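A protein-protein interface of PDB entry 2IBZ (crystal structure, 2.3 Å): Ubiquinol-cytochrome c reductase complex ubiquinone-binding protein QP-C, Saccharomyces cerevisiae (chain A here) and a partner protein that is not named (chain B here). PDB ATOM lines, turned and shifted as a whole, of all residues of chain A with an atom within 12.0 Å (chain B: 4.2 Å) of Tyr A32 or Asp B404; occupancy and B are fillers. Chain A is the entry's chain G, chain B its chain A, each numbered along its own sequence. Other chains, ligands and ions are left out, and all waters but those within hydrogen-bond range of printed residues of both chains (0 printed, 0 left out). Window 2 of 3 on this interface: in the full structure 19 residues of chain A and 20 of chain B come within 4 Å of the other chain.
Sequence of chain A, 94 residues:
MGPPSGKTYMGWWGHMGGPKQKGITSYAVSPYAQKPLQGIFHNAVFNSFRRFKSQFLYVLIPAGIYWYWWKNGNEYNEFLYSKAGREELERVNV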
ATOM      1  N   ALA A  28     -19.140 -16.099  -8.971  1.00  0.00           N
ATOM      2  CA  ALA A  28     -17.837 -15.562  -8.614  1.00  0.00           C
ATOM      3  C   ALA A  28     -17.064 -16.602  -7.799  1.00  0.00           C
ATOM      4  O   ALA A  28     -17.651 -17.523  -7.234  1.00  0.00           O
ATOM      5  CB  ALA A  28     -17.986 -14.239  -7.825  1.00  0.00           C
ATOM      6  N   VAL A  29     -15.756 -16.401  -7.691  1.00  0.00           N
ATOM      7  CA  VAL A  29     -14.891 -17.316  -6.975  1.00  0.00           C
ATOM      8  C   VAL A  29     -13.973 -16.539  -6.038  1.00  0.00           C
ATOM      9  O   VAL A  29     -13.392 -15.521  -6.424  1.00  0.00           O
ATOM     10  CB  VAL A  29     -14.030 -18.148  -7.978  1.00  0.00           C
ATOM     11  CG1 VAL A  29     -12.924 -18.893  -7.246  1.00  0.00           C
ATOM     12  CG2 VAL A  29     -14.912 -19.151  -8.718  1.00  0.00           C
ATOM     13  N   SER A  30     -13.825 -17.045  -4.820  1.00  0.00           N
ATOM     14  CA  SER A  30     -12.989 -16.411  -3.821  1.00  0.00           C
ATOM     15  C   SER A  30     -11.597 -16.074  -4.327  1.00  0.00           C
ATOM     16  O   SER A  30     -10.977 -16.860  -5.054  1.00  0.00           O
ATOM     17  CB  SER A  30     -12.858 -17.303  -2.584  1.00  0.00           C
ATOM     18  OG  SER A  30     -11.885 -16.793  -1.681  1.00  0.00           O
ATOM     19  N   PRO A  31     -11.121 -14.859  -4.007  1.00  0.00           N
ATOM     20  CA  PRO A  31      -9.794 -14.392  -4.403  1.00  0.00           C
ATOM     21  C   PRO A  31      -8.766 -15.326  -3.788  1.00  0.00           C
ATOM     22  O   PRO A  31      -7.666 -15.469  -4.303  1.00  0.00           O
ATOM     23  CB  PRO A  31      -9.724 -13.010  -3.760  1.00  0.00           C
ATOM     24  CG  PRO A  31     -11.137 -12.531  -3.898  1.00  0.00           C
ATOM     25  CD  PRO A  31     -11.924 -13.746  -3.462  1.00  0.00           C
ATOM     26  N   TYR A  32      -9.136 -15.959  -2.679  1.00  0.00           N
ATOM     27  CA  TYR A  32      -8.244 -16.887  -1.990  1.00  0.00           C
ATOM     28  C   TYR A  32      -7.944 -18.121  -2.837  1.00  0.00           C
ATOM     29  O   TYR A  32      -6.810 -18.605  -2.863  1.00  0.00           O
ATOM     30  CB  TYR A  32      -8.845 -17.318  -0.653  1.00  0.00           C
ATOM     31  CG  TYR A  32      -8.695 -16.301   0.446  1.00  0.00           C
ATOM     32  CD1 TYR A  32      -9.707 -15.370   0.710  1.00  0.00           C
ATOM     33  CD2 TYR A  32      -7.557 -16.288   1.251  1.00  0.00           C
ATOM     34  CE1 TYR A  32      -9.590 -14.460   1.757  1.00  0.00           C
ATOM     35  CE2 TYR A  32      -7.427 -15.373   2.302  1.00  0.00           C
ATOM     36  CZ  TYR A  32      -8.447 -14.468   2.552  1.00  0.00           C
ATOM     37  OH  TYR A  32      -8.344 -13.604   3.628  1.00  0.00           O
ATOM     38  N   ALA A  33      -8.961 -18.581  -3.561  1.00  0.00           N
ATOM     39  CA  ALA A  33      -8.861 -19.752  -4.422  1.00  0.00           C
ATOM     40  C   ALA A  33      -8.245 -19.450  -5.786  1.00  0.00           C
ATOM     41  O   ALA A  33      -8.043 -20.357  -6.591  1.00  0.00           O
ATOM     42  CB  ALA A  33     -10.246 -20.362  -4.613  1.00  0.00           C
ATOM     43  N   GLN A  34      -7.962 -18.179  -6.053  1.00  0.00           N
ATOM     44  CA  GLN A  34      -7.406 -17.793  -7.338  1.00  0.00           C
ATOM     45  C   GLN A  34      -5.895 -17.766  -7.376  1.00  0.00           C
ATOM     46  O   GLN A  34      -5.225 -17.602  -6.355  1.00  0.00           O
ATOM     47  CB  GLN A  34      -7.977 -16.450  -7.796  1.00  0.00           C
ATOM     48  CG  GLN A  34      -9.492 -16.454  -7.937  1.00  0.00           C
ATOM     49  CD  GLN A  34     -10.042 -15.152  -8.491  1.00  0.00           C
ATOM     50  OE1 GLN A  34      -9.388 -14.478  -9.285  1.00  0.00           O
ATOM     51  NE2 GLN A  34     -11.259 -14.804  -8.088  1.00  0.00           N
ATOM     52  N   LYS A  35      -5.373 -17.948  -8.580  1.00  0.00           N
ATOM     53  CA  LYS A  35      -3.944 -17.968  -8.834  1.00  0.00           C
ATOM     54  C   LYS A  35      -3.347 -16.626  -8.416  1.00  0.00           C
ATOM     55  O   LYS A  35      -3.707 -15.582  -8.965  1.00  0.00           O
ATOM     56  CB  LYS A  35      -3.720 -18.238 -10.326  1.00  0.00           C
ATOM     57  CG  LYS A  35      -2.385 -18.866 -10.688  1.00  0.00           C
ATOM     58  CD  LYS A  35      -2.544 -19.845 -11.856  1.00  0.00           C
ATOM     59  CE  LYS A  35      -3.238 -19.203 -13.061  1.00  0.00           C
ATOM     60  NZ  LYS A  35      -3.425 -20.161 -14.193  1.00  0.00           N
ATOM     61  N   PRO A  36      -2.451 -16.636  -7.410  1.00  0.00           N
ATOM     62  CA  PRO A  36      -1.794 -15.426  -6.900  1.00  0.00           C
ATOM     63  C   PRO A  36      -1.208 -14.580  -8.022  1.00  0.00           C
ATOM     64  O   PRO A  36      -0.622 -15.102  -8.971  1.00  0.00           O
ATOM     65  CB  PRO A  36      -0.717 -15.981  -5.964  1.00  0.00           C
ATOM     66  CG  PRO A  36      -0.488 -17.383  -6.467  1.00  0.00           C
ATOM     67  CD  PRO A  36      -1.885 -17.836  -6.774  1.00  0.00           C
ATOM     68  N   LEU A  37      -1.385 -13.270  -7.899  1.00  0.00           N
ATOM     69  CA  LEU A  37      -0.933 -12.293  -8.886  1.00  0.00           C
ATOM     70  C   LEU A  37       0.427 -12.538  -9.547  1.00  0.00           C
ATOM     71  O   LEU A  37       1.484 -12.246  -8.980  1.00  0.00           O
ATOM     72  CB  LEU A  37      -0.997 -10.891  -8.279  1.00  0.00           C
ATOM     73  CG  LEU A  37      -2.331 -10.593  -7.580  1.00  0.00           C
ATOM     74  CD1 LEU A  37      -2.229  -9.280  -6.851  1.00  0.00           C
ATOM     75  CD2 LEU A  37      -3.494 -10.586  -8.575  1.00  0.00           C
ATOM     76  N   PHE B 218     -14.107 -28.819  -2.396  1.00  0.00           N
ATOM     77  CA  PHE B 218     -14.814 -27.586  -2.065  1.00  0.00           C
ATOM     78  C   PHE B 218     -14.085 -26.386  -2.672  1.00  0.00           C
ATOM     79  O   PHE B 218     -12.856 -26.295  -2.634  1.00  0.00           O
ATOM     80  CB  PHE B 218     -14.911 -27.437  -0.536  1.00  0.00           C
ATOM     81  CG  PHE B 218     -15.640 -26.203  -0.081  1.00  0.00           C
ATOM     82  CD1 PHE B 218     -17.007 -26.241   0.163  1.00  0.00           C
ATOM     83  CD2 PHE B 218     -14.954 -25.005   0.111  1.00  0.00           C
ATOM     84  CE1 PHE B 218     -17.678 -25.103   0.592  1.00  0.00           C
ATOM     85  CE2 PHE B 218     -15.611 -23.863   0.539  1.00  0.00           C
ATOM     86  CZ  PHE B 218     -16.975 -23.908   0.780  1.00  0.00           C
ATOM     87  N   GLY B 220     -14.408 -22.201  -2.620  1.00  0.00           N
ATOM     88  CA  GLY B 220     -15.058 -21.003  -2.090  1.00  0.00           C
ATOM     89  C   GLY B 220     -15.570 -20.180  -3.251  1.00  0.00           C
ATOM     90  O   GLY B 220     -14.783 -19.744  -4.080  1.00  0.00           O
ATOM     91  N   VAL B 239     -19.346 -23.583   4.881  1.00  0.00           N
ATOM     92  CA  VAL B 239     -17.915 -23.827   4.738  1.00  0.00           C
ATOM     93  C   VAL B 239     -17.765 -25.330   4.424  1.00  0.00           C
ATOM     94  O   VAL B 239     -18.759 -26.081   4.458  1.00  0.00           O
ATOM     95  CB  VAL B 239     -17.138 -23.498   6.039  1.00  0.00           C
ATOM     96  CG1 VAL B 239     -17.254 -22.014   6.370  1.00  0.00           C
ATOM     97  CG2 VAL B 239     -17.644 -24.353   7.209  1.00  0.00           C
ATOM     98  N   ASP B 402     -11.376 -17.987   9.409  1.00  0.00           N
ATOM     99  CA  ASP B 402     -10.667 -17.456   8.246  1.00  0.00           C
ATOM    100  C   ASP B 402     -10.600 -18.496   7.127  1.00  0.00           C
ATOM    101  O   ASP B 402      -9.554 -18.738   6.540  1.00  0.00           O
ATOM    102  CB  ASP B 402      -9.265 -16.992   8.659  1.00  0.00           C
ATOM    103  CG  ASP B 402      -8.592 -16.119   7.614  1.00  0.00           C
ATOM    104  OD1 ASP B 402      -9.271 -15.601   6.706  1.00  0.00           O
ATOM    105  OD2 ASP B 402      -7.364 -15.933   7.720  1.00  0.00           O
ATOM    106  N   GLN B 403     -11.748 -19.088   6.829  1.00  0.00           N
ATOM    107  CA  GLN B 403     -11.863 -20.101   5.794  1.00  0.00           C
ATOM    108  C   GLN B 403     -12.820 -19.614   4.726  1.00  0.00           C
ATOM    109  O   GLN B 403     -13.745 -18.845   5.016  1.00  0.00           O
ATOM    110  CB  GLN B 403     -12.425 -21.410   6.377  1.00  0.00           C
ATOM    111  CG  GLN B 403     -11.486 -22.145   7.312  1.00  0.00           C
ATOM    112  CD  GLN B 403     -10.190 -22.552   6.641  1.00  0.00           C
ATOM    113  OE1 GLN B 403     -10.175 -22.955   5.478  1.00  0.00           O
ATOM    114  NE2 GLN B 403      -9.086 -22.443   7.378  1.00  0.00           N
ATOM    115  N   ASP B 404     -12.615 -20.090   3.501  1.00  0.00           N
ATOM    116  CA  ASP B 404     -13.468 -19.731   2.386  1.00  0.00           C
ATOM    117  C   ASP B 404     -14.875 -20.196   2.655  1.00  0.00           C
ATOM    118  O   ASP B 404     -15.088 -21.114   3.424  1.00  0.00           O
ATOM    119  CB  ASP B 404     -12.971 -20.396   1.102  1.00  0.00           C
ATOM    120  CG  ASP B 404     -11.990 -19.541   0.340  1.00  0.00           C
ATOM    121  OD1 ASP B 404     -11.271 -20.084  -0.535  1.00  0.00           O
ATOM    122  OD2 ASP B 404     -11.963 -18.320   0.584  1.00  0.00           O
ATOM    123  N   ILE B 405     -15.839 -19.573   1.998  1.00  0.00           N
ATOM    124  CA  ILE B 405     -17.241 -19.943   2.158  1.00  0.00           C
ATOM    125  C   ILE B 405     -17.861 -20.096   0.784  1.00  0.00           C
ATOM    126  O   ILE B 405     -17.259 -19.740  -0.232  1.00  0.00           O
ATOM    127  CB  ILE B 405     -18.042 -18.862   2.912  1.00  0.00           C
ATOM    128  CG1 ILE B 405     -17.941 -17.531   2.156  1.00  0.00           C
ATOM    129  CG2 ILE B 405     -17.549 -18.743   4.351  1.00  0.00           C
ATOM    130  CD1 ILE B 405     -18.527 -16.356   2.881  1.00  0.00           C
ATOM    131  N   TYR B 419     -18.948 -10.875  -1.886  1.00  0.00           N
ATOM    132  CA  TYR B 419     -18.257 -12.009  -1.324  1.00  0.00           C
ATOM    133  C   TYR B 419     -17.256 -11.624  -0.253  1.00  0.00           C
ATOM    134  O   TYR B 419     -17.365 -12.097   0.874  1.00  0.00           O
ATOM    135  CB  TYR B 419     -17.565 -12.810  -2.432  1.00  0.00           C
ATOM    136  CG  TYR B 419     -16.992 -14.123  -1.941  1.00  0.00           C
ATOM    137  CD1 TYR B 419     -17.791 -15.272  -1.879  1.00  0.00           C
ATOM    138  CD2 TYR B 419     -15.658 -14.214  -1.516  1.00  0.00           C
ATOM    139  CE1 TYR B 419     -17.279 -16.480  -1.409  1.00  0.00           C
ATOM    140  CE2 TYR B 419     -15.135 -15.416  -1.035  1.00  0.00           C
ATOM    141  CZ  TYR B 419     -15.957 -16.548  -0.988  1.00  0.00           C
ATOM    142  OH  TYR B 419     -15.464 -17.740  -0.509  1.00  0.00           O
ATOM    143  N   ARG B 423     -16.846 -12.914   3.509  1.00  0.00           N
ATOM    144  CA  ARG B 423     -15.641 -13.684   3.808  1.00  0.00           C
ATOM    145  C   ARG B 423     -14.789 -13.071   4.930  1.00  0.00           C
ATOM    146  O   ARG B 423     -14.252 -13.793   5.768  1.00  0.00           O
ATOM    147  CB  ARG B 423     -14.846 -13.926   2.504  1.00  0.00           C
ATOM    148  CG  ARG B 423     -13.454 -14.529   2.636  1.00  0.00           C
ATOM    149  CD  ARG B 423     -13.426 -15.962   3.176  1.00  0.00           C
ATOM    150  NE  ARG B 423     -12.283 -16.105   4.086  1.00  0.00           N
ATOM    151  CZ  ARG B 423     -11.160 -16.742   3.781  1.00  0.00           C
ATOM    152  NH1 ARG B 423     -10.159 -16.797   4.632  1.00  0.00           N
ATOM    153  NH2 ARG B 423     -11.059 -17.394   2.648  1.00  0.00           N
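Of the 9 printed residues of chain B, 5 touch a printed residue of chain A.
Printed residues of chain B that touch a printed residue of chain A: Gly B220, Asp B402, Asp B404, Tyr B419 and Arg B423.
Hydrophobic or aromatic side chains of chain B within 4 Å of the printed part of chain A: Tyr B419.
Of the 10 printed residues of chain A, 3 touch a printed residue of chain B.
Hydrophobic or aromatic side chains of chain A within 4 Å of the printed part of chain B: Val A29 and Tyr A32.
Among the printed residues, 7 pairs touch across the chains.
The guanidinium group (NH1) of Arg B423 is in salt-bridge range of the side-chain carboxylate (OD1) of Asp B402, 2.6 Å away.
O of Gln B403 is in hydrogen-bond range of NE of Arg B423 (3.2 Å).
OD2 of Asp B404 lies within salt-bridge range of NH2 of Arg B423.
O of Ile B405 sits at hydrogen-bond distance from OH of Tyr B419 (2.7 Å).
O of Val A29 sits at hydrogen-bond distance from NE2 of Gln A34 (2.8 Å).
The side-chain hydroxyl of Ser A30 sits close to the backbone NH of Tyr A32, at 3.0 Å.
Of the printed residues of chain B, Val A29 touches Gly B220 (3.8 Å).
Pro A31 touches none of the printed residues of chain B.
Tyr A32 touches just these residues of chain B: Asp B402 (3.8 Å), Asp B404 (3.5 Å) and Arg B423 (3.1 Å).
Pro A36 touches none of the printed residues of chain B.
No residue of chain A comes within 4 Å of Val B239.
Asp B402 touches just one residue of chain A: Tyr A32.
No residue of chain A comes within 4 Å of Gln B403.
Asp B404 touches just these residues of chain A: Ser A30 (2.7 Å) and Tyr A32 (3.5 Å).
No residue of chain A comes within 4 Å of Ile B405.
Of the printed residues of chain A, Tyr B419 touches Ser A30.
Of chain A, only Tyr A32 (3.1 Å) comes within 4 Å of Arg B423.
The nearest printed residue of chain B that does not touch Tyr A32 is Tyr B419 (5.7 Å).
The nearest printed residue of chain B that does not touch Val A29 is Tyr B419 (5.3 Å).
The backbone carbonyl oxygen (O) of Gly B220 lies within hydrogen-bond range of the backbone NH (N) of Ser A30 (3.0 Å).
The side-chain carboxylate of Asp B404 sits at hydrogen-bond distance from the side-chain hydroxyl of Ser A30 (2.7 Å).
Among the printed residues, pairs that only touch across the chains: Val A29 with Gly B220 (3.8 Å), Ser A30 with Tyr B419 (3.3 Å), Tyr A32 with Asp B402 (3.8 Å), Tyr A32 with Asp B404 (3.5 Å) and Tyr A32 with Arg B423 (3.1 Å).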
